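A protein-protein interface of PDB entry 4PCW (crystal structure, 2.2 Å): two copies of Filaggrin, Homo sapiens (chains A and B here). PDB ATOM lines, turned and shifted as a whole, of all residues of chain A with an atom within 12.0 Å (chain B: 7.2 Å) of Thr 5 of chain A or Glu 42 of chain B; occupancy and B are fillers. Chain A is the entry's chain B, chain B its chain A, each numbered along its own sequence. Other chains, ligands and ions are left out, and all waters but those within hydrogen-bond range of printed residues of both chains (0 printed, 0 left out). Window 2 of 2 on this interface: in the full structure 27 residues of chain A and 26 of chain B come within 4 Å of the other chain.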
ATOM      1  N   SER A   4      30.954   6.054  15.465  1.00  0.00           N
ATOM      2  CA  SER A   4      29.551   5.602  15.697  1.00  0.00           C
ATOM      3  C   SER A   4      28.764   5.554  14.389  1.00  0.00           C
ATOM      4  O   SER A   4      29.092   6.254  13.432  1.00  0.00           O
ATOM      5  CB  SER A   4      28.853   6.526  16.697  1.00  0.00           C
ATOM      6  OG  SER A   4      28.922   7.879  16.278  1.00  0.00           O
ATOM      7  N   THR A   5      27.728   4.719  14.355  1.00  0.00           N
ATOM      8  CA  THR A   5      26.866   4.596  13.182  1.00  0.00           C
ATOM      9  C   THR A   5      25.675   5.542  13.277  1.00  0.00           C
ATOM     10  O   THR A   5      25.483   6.215  14.292  1.00  0.00           O
ATOM     11  CB  THR A   5      26.334   3.160  13.013  1.00  0.00           C
ATOM     12  OG1 THR A   5      25.559   2.794  14.162  1.00  0.00           O
ATOM     13  CG2 THR A   5      27.478   2.177  12.841  1.00  0.00           C
ATOM     14  N   LEU A   6      24.877   5.592  12.218  1.00  0.00           N
ATOM     15  CA  LEU A   6      23.657   6.383  12.234  1.00  0.00           C
ATOM     16  C   LEU A   6      22.664   5.786  13.217  1.00  0.00           C
ATOM     17  O   LEU A   6      21.978   6.508  13.941  1.00  0.00           O
ATOM     18  CB  LEU A   6      23.025   6.454  10.843  1.00  0.00           C
ATOM     19  CG  LEU A   6      21.805   7.373  10.746  1.00  0.00           C
ATOM     20  CD1 LEU A   6      22.217   8.832  10.874  1.00  0.00           C
ATOM     21  CD2 LEU A   6      21.055   7.141   9.453  1.00  0.00           C
ATOM     22  N   LEU A   7      22.591   4.460  13.239  1.00  0.00           N
ATOM     23  CA  LEU A   7      21.604   3.767  14.055  1.00  0.00           C
ATOM     24  C   LEU A   7      21.885   3.945  15.546  1.00  0.00           C
ATOM     25  O   LEU A   7      20.962   3.959  16.361  1.00  0.00           O
ATOM     26  CB  LEU A   7      21.576   2.281  13.694  1.00  0.00           C
ATOM     27  CG  LEU A   7      20.285   1.518  14.004  1.00  0.00           C
ATOM     28  CD1 LEU A   7      19.105   2.077  13.219  1.00  0.00           C
ATOM     29  CD2 LEU A   7      20.471   0.044  13.697  1.00  0.00           C
ATOM     30  N   GLU A   8      23.158   4.084  15.900  1.00  0.00           N
ATOM     31  CA  GLU A   8      23.537   4.350  17.283  1.00  0.00           C
ATOM     32  C   GLU A   8      23.104   5.756  17.696  1.00  0.00           C
ATOM     33  O   GLU A   8      22.626   5.969  18.811  1.00  0.00           O
ATOM     34  CB  GLU A   8      25.046   4.184  17.466  1.00  0.00           C
ATOM     35  CG  GLU A   8      25.540   2.755  17.280  1.00  0.00           C
ATOM     36  CD  GLU A   8      25.896   2.079  18.593  1.00  0.00           C
ATOM     37  OE1 GLU A   8      26.734   2.627  19.340  1.00  0.00           O
ATOM     38  OE2 GLU A   8      25.338   0.998  18.878  1.00  0.00           O
ATOM     39  N   ASN A   9      23.271   6.709  16.783  1.00  0.00           N
ATOM     40  CA  ASN A   9      22.889   8.096  17.029  1.00  0.00           C
ATOM     41  C   ASN A   9      21.380   8.272  17.132  1.00  0.00           C
ATOM     42  O   ASN A   9      20.892   9.059  17.944  1.00  0.00           O
ATOM     43  CB  ASN A   9      23.441   8.995  15.921  1.00  0.00           C
ATOM     44  CG  ASN A   9      24.934   9.213  16.042  1.00  0.00           C
ATOM     45  OD1 ASN A   9      25.437   9.561  17.111  1.00  0.00           O
ATOM     46  ND2 ASN A   9      25.654   9.001  14.947  1.00  0.00           N
ATOM     47  N   ILE A  10      20.645   7.541  16.302  1.00  0.00           N
ATOM     48  CA  ILE A  10      19.190   7.579  16.346  1.00  0.00           C
ATOM     49  C   ILE A  10      18.704   7.063  17.698  1.00  0.00           C
ATOM     50  O   ILE A  10      17.845   7.673  18.332  1.00  0.00           O
ATOM     51  CB  ILE A  10      18.575   6.749  15.200  1.00  0.00           C
ATOM     52  CG1 ILE A  10      18.790   7.470  13.865  1.00  0.00           C
ATOM     53  CG2 ILE A  10      17.084   6.512  15.438  1.00  0.00           C
ATOM     54  CD1 ILE A  10      18.457   6.640  12.643  1.00  0.00           C
ATOM     55  N   PHE A  11      19.264   5.942  18.139  1.00  0.00           N
ATOM     56  CA  PHE A  11      18.882   5.353  19.418  1.00  0.00           C
ATOM     57  C   PHE A  11      19.328   6.211  20.601  1.00  0.00           C
ATOM     58  O   PHE A  11      18.673   6.225  21.645  1.00  0.00           O
ATOM     59  CB  PHE A  11      19.459   3.943  19.546  1.00  0.00           C
ATOM     60  CG  PHE A  11      18.506   2.866  19.122  1.00  0.00           C
ATOM     61  CD1 PHE A  11      17.598   2.336  20.022  1.00  0.00           C
ATOM     62  CD2 PHE A  11      18.508   2.393  17.822  1.00  0.00           C
ATOM     63  CE1 PHE A  11      16.714   1.349  19.637  1.00  0.00           C
ATOM     64  CE2 PHE A  11      17.627   1.405  17.429  1.00  0.00           C
ATOM     65  CZ  PHE A  11      16.728   0.883  18.338  1.00  0.00           C
ATOM     66  N   ALA A  12      20.441   6.919  20.441  1.00  0.00           N
ATOM     67  CA  ALA A  12      20.905   7.842  21.471  1.00  0.00           C
ATOM     68  C   ALA A  12      19.882   8.956  21.671  1.00  0.00           C
ATOM     69  O   ALA A  12      19.577   9.339  22.801  1.00  0.00           O
ATOM     70  CB  ALA A  12      22.262   8.418  21.097  1.00  0.00           C
ATOM     71  N   ILE A  13      19.349   9.464  20.565  1.00  0.00           N
ATOM     72  CA  ILE A  13      18.333  10.505  20.614  1.00  0.00           C
ATOM     73  C   ILE A  13      17.052   9.965  21.245  1.00  0.00           C
ATOM     74  O   ILE A  13      16.389  10.665  22.010  1.00  0.00           O
ATOM     75  CB  ILE A  13      18.034  11.063  19.205  1.00  0.00           C
ATOM     76  CG1 ILE A  13      19.261  11.804  18.668  1.00  0.00           C
ATOM     77  CG2 ILE A  13      16.834  12.013  19.231  1.00  0.00           C
ATOM     78  CD1 ILE A  13      19.188  12.137  17.194  1.00  0.00           C
ATOM     79  N   ILE A  14      16.709   8.721  20.923  1.00  0.00           N
ATOM     80  CA  ILE A  14      15.526   8.080  21.487  1.00  0.00           C
ATOM     81  C   ILE A  14      15.667   7.907  22.999  1.00  0.00           C
ATOM     82  O   ILE A  14      14.756   8.240  23.756  1.00  0.00           O
ATOM     83  CB  ILE A  14      15.265   6.705  20.833  1.00  0.00           C
ATOM     84  CG1 ILE A  14      14.826   6.888  19.378  1.00  0.00           C
ATOM     85  CG2 ILE A  14      14.185   5.930  21.596  1.00  0.00           C
ATOM     86  CD1 ILE A  14      14.765   5.601  18.571  1.00  0.00           C
ATOM     87  N   ASN A  15      16.810   7.382  23.432  1.00  0.00           N
ATOM     88  CA  ASN A  15      17.051   7.121  24.847  1.00  0.00           C
ATOM     89  C   ASN A  15      17.237   8.400  25.652  1.00  0.00           C
ATOM     90  O   ASN A  15      16.999   8.421  26.860  1.00  0.00           O
ATOM     91  CB  ASN A  15      18.275   6.222  25.014  1.00  0.00           C
ATOM     92  CG  ASN A  15      18.046   4.825  24.476  1.00  0.00           C
ATOM     93  OD1 ASN A  15      16.965   4.256  24.633  1.00  0.00           O
ATOM     94  ND2 ASN A  15      19.061   4.265  23.831  1.00  0.00           N
ATOM     95  N   ASN B   9      25.314  13.807  18.779  1.00  0.00           N
ATOM     96  CA  ASN B   9      24.574  12.945  17.872  1.00  0.00           C
ATOM     97  C   ASN B   9      24.219  13.685  16.586  1.00  0.00           C
ATOM     98  O   ASN B   9      24.314  13.124  15.495  1.00  0.00           O
ATOM     99  CB  ASN B   9      23.310  12.416  18.552  1.00  0.00           C
ATOM    100  CG  ASN B   9      23.619  11.515  19.733  1.00  0.00           C
ATOM    101  OD1 ASN B   9      23.160  11.755  20.848  1.00  0.00           O
ATOM    102  ND2 ASN B   9      24.408  10.474  19.491  1.00  0.00           N
ATOM    103  N   ALA B  12      27.219  14.126  14.459  1.00  0.00           N
ATOM    104  CA  ALA B  12      27.562  12.819  13.908  1.00  0.00           C
ATOM    105  C   ALA B  12      26.700  12.507  12.688  1.00  0.00           C
ATOM    106  O   ALA B  12      27.183  11.949  11.700  1.00  0.00           O
ATOM    107  CB  ALA B  12      27.400  11.740  14.961  1.00  0.00           C
ATOM    108  N   ILE B  13      25.425  12.871  12.760  1.00  0.00           N
ATOM    109  CA  ILE B  13      24.516  12.676  11.638  1.00  0.00           C
ATOM    110  C   ILE B  13      24.954  13.550  10.464  1.00  0.00           C
ATOM    111  O   ILE B  13      24.978  13.099   9.320  1.00  0.00           O
ATOM    112  CB  ILE B  13      23.059  12.997  12.033  1.00  0.00           C
ATOM    113  CG1 ILE B  13      22.543  11.947  13.018  1.00  0.00           C
ATOM    114  CG2 ILE B  13      22.154  13.028  10.800  1.00  0.00           C
ATOM    115  CD1 ILE B  13      21.228  12.306  13.694  1.00  0.00           C
ATOM    116  N   LEU B  16      28.164  12.190   8.999  1.00  0.00           N
ATOM    117  CA  LEU B  16      27.851  10.941   8.325  1.00  0.00           C
ATOM    118  C   LEU B  16      27.356  11.222   6.910  1.00  0.00           C
ATOM    119  O   LEU B  16      27.800  10.595   5.948  1.00  0.00           O
ATOM    120  CB  LEU B  16      26.803  10.158   9.120  1.00  0.00           C
ATOM    121  CG  LEU B  16      26.300   8.843   8.522  1.00  0.00           C
ATOM    122  CD1 LEU B  16      26.081   7.833   9.630  1.00  0.00           C
ATOM    123  CD2 LEU B  16      25.013   9.051   7.733  1.00  0.00           C
ATOM    124  N   PHE B  17      26.443  12.182   6.795  1.00  0.00           N
ATOM    125  CA  PHE B  17      25.859  12.551   5.511  1.00  0.00           C
ATOM    126  C   PHE B  17      26.916  13.110   4.571  1.00  0.00           C
ATOM    127  O   PHE B  17      26.966  12.751   3.394  1.00  0.00           O
ATOM    128  CB  PHE B  17      24.737  13.574   5.716  1.00  0.00           C
ATOM    129  CG  PHE B  17      24.176  14.134   4.436  1.00  0.00           C
ATOM    130  CD1 PHE B  17      23.136  13.495   3.780  1.00  0.00           C
ATOM    131  CD2 PHE B  17      24.676  15.311   3.900  1.00  0.00           C
ATOM    132  CE1 PHE B  17      22.613  14.014   2.607  1.00  0.00           C
ATOM    133  CE2 PHE B  17      24.157  15.833   2.728  1.00  0.00           C
ATOM    134  CZ  PHE B  17      23.125  15.184   2.081  1.00  0.00           C
ATOM    135  N   GLN B  19      30.032  12.593   4.551  1.00  0.00           N
ATOM    136  CA  GLN B  19      31.019  11.585   4.187  1.00  0.00           C
ATOM    137  C   GLN B  19      30.685  10.960   2.837  1.00  0.00           C
ATOM    138  O   GLN B  19      31.582  10.608   2.069  1.00  0.00           O
ATOM    139  CB  GLN B  19      31.099  10.496   5.262  1.00  0.00           C
ATOM    140  CG  GLN B  19      32.081   9.372   4.947  1.00  0.00           C
ATOM    141  CD  GLN B  19      32.071   8.278   5.995  1.00  0.00           C
ATOM    142  OE1 GLN B  19      31.748   8.517   7.158  1.00  0.00           O
ATOM    143  NE2 GLN B  19      32.423   7.064   5.584  1.00  0.00           N
ATOM    144  N   TYR B  20      29.394  10.831   2.552  1.00  0.00           N
ATOM    145  CA  TYR B  20      28.946  10.163   1.338  1.00  0.00           C
ATOM    146  C   TYR B  20      28.515  11.159   0.267  1.00  0.00           C
ATOM    147  O   TYR B  20      28.601  10.867  -0.924  1.00  0.00           O
ATOM    148  CB  TYR B  20      27.804   9.197   1.659  1.00  0.00           C
ATOM    149  CG  TYR B  20      28.220   8.066   2.576  1.00  0.00           C
ATOM    150  CD1 TYR B  20      28.855   6.938   2.075  1.00  0.00           C
ATOM    151  CD2 TYR B  20      27.984   8.131   3.942  1.00  0.00           C
ATOM    152  CE1 TYR B  20      29.240   5.903   2.910  1.00  0.00           C
ATOM    153  CE2 TYR B  20      28.364   7.103   4.783  1.00  0.00           C
ATOM    154  CZ  TYR B  20      28.992   5.992   4.263  1.00  0.00           C
ATOM    155  OH  TYR B  20      29.371   4.968   5.100  1.00  0.00           O
ATOM    156  N   GLU B  37      25.872   3.567  -1.473  1.00  0.00           N
ATOM    157  CA  GLU B  37      27.033   3.428  -0.601  1.00  0.00           C
ATOM    158  C   GLU B  37      26.616   3.579   0.859  1.00  0.00           C
ATOM    159  O   GLU B  37      26.930   2.736   1.700  1.00  0.00           O
ATOM    160  CB  GLU B  37      28.097   4.473  -0.955  1.00  0.00           C
ATOM    161  CG  GLU B  37      29.377   3.914  -1.568  1.00  0.00           C
ATOM    162  CD  GLU B  37      30.631   4.354  -0.821  1.00  0.00           C
ATOM    163  OE1 GLU B  37      31.624   4.708  -1.489  1.00  0.00           O
ATOM    164  OE2 GLU B  37      30.629   4.338   0.429  1.00  0.00           O
ATOM    165  N   LEU B  38      25.895   4.657   1.146  1.00  0.00           N
ATOM    166  CA  LEU B  38      25.432   4.952   2.497  1.00  0.00           C
ATOM    167  C   LEU B  38      24.505   3.853   3.015  1.00  0.00           C
ATOM    168  O   LEU B  38      24.652   3.386   4.148  1.00  0.00           O
ATOM    169  CB  LEU B  38      24.718   6.306   2.515  1.00  0.00           C
ATOM    170  CG  LEU B  38      24.624   7.042   3.853  1.00  0.00           C
ATOM    171  CD1 LEU B  38      24.351   8.521   3.620  1.00  0.00           C
ATOM    172  CD2 LEU B  38      23.546   6.447   4.736  1.00  0.00           C
ATOM    173  N   LEU B  39      23.558   3.442   2.178  1.00  0.00           N
ATOM    174  CA  LEU B  39      22.604   2.395   2.538  1.00  0.00           C
ATOM    175  C   LEU B  39      23.291   1.053   2.797  1.00  0.00           C
ATOM    176  O   LEU B  39      22.716   0.167   3.427  1.00  0.00           O
ATOM    177  CB  LEU B  39      21.555   2.223   1.433  1.00  0.00           C
ATOM    178  CG  LEU B  39      20.612   3.390   1.116  1.00  0.00           C
ATOM    179  CD1 LEU B  39      19.680   3.022  -0.032  1.00  0.00           C
ATOM    180  CD2 LEU B  39      19.822   3.810   2.333  1.00  0.00           C
ATOM    181  N   GLU B  40      24.518   0.905   2.306  1.00  0.00           N
ATOM    182  CA  GLU B  40      25.236  -0.364   2.405  1.00  0.00           C
ATOM    183  C   GLU B  40      26.131  -0.450   3.639  1.00  0.00           C
ATOM    184  O   GLU B  40      26.561  -1.540   4.017  1.00  0.00           O
ATOM    185  CB  GLU B  40      26.079  -0.589   1.144  1.00  0.00           C
ATOM    186  CG  GLU B  40      25.323  -1.272   0.005  1.00  0.00           C
ATOM    187  CD  GLU B  40      26.124  -1.329  -1.284  1.00  0.00           C
ATOM    188  OE1 GLU B  40      27.153  -0.628  -1.384  1.00  0.00           O
ATOM    189  OE2 GLU B  40      25.723  -2.077  -2.200  1.00  0.00           O
ATOM    190  N   LYS B  41      26.399   0.690   4.272  1.00  0.00           N
ATOM    191  CA  LYS B  41      27.353   0.743   5.377  1.00  0.00           C
ATOM    192  C   LYS B  41      26.722   1.180   6.696  1.00  0.00           C
ATOM    193  O   LYS B  41      26.709   0.422   7.665  1.00  0.00           O
ATOM    194  CB  LYS B  41      28.507   1.684   5.026  1.00  0.00           C
ATOM    195  CG  LYS B  41      29.248   1.295   3.758  1.00  0.00           C
ATOM    196  CD  LYS B  41      30.436   2.208   3.509  1.00  0.00           C
ATOM    197  CE  LYS B  41      31.109   1.902   2.180  1.00  0.00           C
ATOM    198  NZ  LYS B  41      31.622   0.506   2.110  1.00  0.00           N
ATOM    199  N   GLU B  42      26.201   2.403   6.730  1.00  0.00           N
ATOM    200  CA  GLU B  42      25.767   3.021   7.981  1.00  0.00           C
ATOM    201  C   GLU B  42      24.506   2.386   8.569  1.00  0.00           C
ATOM    202  O   GLU B  42      24.302   2.402   9.784  1.00  0.00           O
ATOM    203  CB  GLU B  42      25.539   4.514   7.764  1.00  0.00           C
ATOM    204  CG  GLU B  42      26.812   5.277   7.443  1.00  0.00           C
ATOM    205  CD  GLU B  42      27.823   5.228   8.572  1.00  0.00           C
ATOM    206  OE1 GLU B  42      27.410   5.031   9.736  1.00  0.00           O
ATOM    207  OE2 GLU B  42      29.032   5.381   8.296  1.00  0.00           O
ATOM    208  N   PHE B  43      23.658   1.845   7.703  1.00  0.00           N
ATOM    209  CA  PHE B  43      22.510   1.058   8.139  1.00  0.00           C
ATOM    210  C   PHE B  43      22.140   0.085   7.027  1.00  0.00           C
ATOM    211  O   PHE B  43      21.725   0.490   5.945  1.00  0.00           O
ATOM    212  CB  PHE B  43      21.325   1.956   8.514  1.00  0.00           C
ATOM    213  CG  PHE B  43      21.075   3.079   7.548  1.00  0.00           C
ATOM    214  CD1 PHE B  43      21.717   4.294   7.702  1.00  0.00           C
ATOM    215  CD2 PHE B  43      20.187   2.926   6.498  1.00  0.00           C
ATOM    216  CE1 PHE B  43      21.484   5.332   6.821  1.00  0.00           C
ATOM    217  CE2 PHE B  43      19.955   3.960   5.614  1.00  0.00           C
ATOM    218  CZ  PHE B  43      20.603   5.164   5.776  1.00  0.00           C
ATOM    219  N   ARG B  44      22.293  -1.204   7.309  1.00  0.00           N
ATOM    220  CA  ARG B  44      22.335  -2.211   6.258  1.00  0.00           C
ATOM    221  C   ARG B  44      21.078  -3.100   6.237  1.00  0.00           C
ATOM    222  O   ARG B  44      19.971  -2.597   6.030  1.00  0.00           O
ATOM    223  CB  ARG B  44      23.605  -3.044   6.434  1.00  0.00           C
ATOM    224  CG  ARG B  44      24.022  -3.750   5.178  1.00  0.00           C
ATOM    225  CD  ARG B  44      24.782  -5.028   5.436  1.00  0.00           C
ATOM    226  NE  ARG B  44      24.481  -6.002   4.395  1.00  0.00           N
ATOM    227  CZ  ARG B  44      24.834  -5.866   3.121  1.00  0.00           C
ATOM    228  NH1 ARG B  44      25.510  -4.795   2.720  1.00  0.00           N
ATOM    229  NH2 ARG B  44      24.509  -6.806   2.244  1.00  0.00           N
ATOM    230  N   ILE B  46      19.643  -4.030   8.481  1.00  0.00           N
ATOM    231  CA  ILE B  46      18.816  -3.310   9.432  1.00  0.00           C
ATOM    232  C   ILE B  46      17.555  -2.758   8.766  1.00  0.00           C
ATOM    233  O   ILE B  46      16.438  -3.020   9.221  1.00  0.00           O
ATOM    234  CB  ILE B  46      19.620  -2.152  10.074  1.00  0.00           C
ATOM    235  CG1 ILE B  46      20.431  -2.661  11.266  1.00  0.00           C
ATOM    236  CG2 ILE B  46      18.710  -1.025  10.544  1.00  0.00           C
ATOM    237  CD1 ILE B  46      21.368  -3.807  10.949  1.00  0.00           C
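The side-chain amide nitrogen (ND2) of Asn 9 of chain B sits at hydrogen-bond distance from the side-chain amide oxygen (OD1) of Asn 9 of chain A (2.7 Å).
The backbone NH (N) of Glu 8 of chain A lies close to the side-chain hydroxyl (OG1) of Thr 5 of chain A, at 3.2 Å. The side-chain amide nitrogen (ND2) of Asn 9 of chain A is in hydrogen-bond range of the backbone carbonyl oxygen (O) of Thr 5 of chain A (2.9 Å). The side-chain carboxylate of Glu 42 of chain B lies within hydrogen-bond range of the side-chain hydroxyl of Tyr 20 of chain B (3.2 Å).
Thr 5 of chain A touches Glu 42 of chain B (CA to OE1, 3.5 Å). CD1 of Leu 6 of chain A touches CG1 of Ile 13 of chain B, at 3.8 Å. Leu 16 of chain B touches Leu 6 of chain A (CD1 to CB, 3.6 Å). Glu 42 of chain B touches Leu 6 of chain A. CD2 of Leu 6 of chain A touches CE1 of Phe 43 of chain B, 3.2 Å away. CD2 of Leu 7 of chain A touches CG1 of Ile 46 of chain B (3.6 Å). ND2 of Asn 9 of chain A touches CB of Ala 12 of chain B, 3.2 Å away. CB of Ala 12 of chain A touches ND2 of Asn 9 of chain B, at 3.4 Å.
Of chain B, only Glu 42 (3.5 Å) comes within 4 Å of Thr 5 of chain A. Glu 42 of chain B touches just these residues of chain A: Thr 5 (3.5 Å) and Leu 6 (3.6 Å). No residue of chain A comes within 4 Å of Leu 38 of chain B. Phe 43 of chain B touches one residue of chain A. Of the printed residues of chain B, Asn 9 of chain A touches Asn 9 and Ala 12. Of the printed residues of chain A, Ile 13 of chain B touches Leu 6 (3.8 Å). Printed residues of chain B within 4 Å of Ala 12 of chain A: Asn 9. The nearest residue of chain B that does not touch Thr 5 of chain A is Leu 16 of chain B (4.3 Å). The nearest residue of chain A that does not touch Glu 42 of chain B is Ser 4 of chain A (4.2 Å).
Of the 12 printed residues of chain A, 5 touch a printed residue of chain B. Hydrophobic or aromatic side chains of chain A that line the printed part of chain B: Leu 6, Leu 7 and Ala 12. Hydrophobic or aromatic side chains of chain B that line the printed part of chain A: Ala 12, Ile 13, Leu 16, Phe 43 and Ile 46. Among the printed residues, 9 pairs touch across the chains.
Asn 9 of chain A touches its own counterpart, Asn 9 of chain B. Asn 9 of chain A touches Ala 12 of chain B, and with the chains exchanged Ala 12 of chain A touches Asn 9 of chain B. Positions printed for both chains: 9, 12 and 13. Of the 9 pairs that touch across the chains among the printed residues, 3 have their exchanged pair printed and touching as well.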
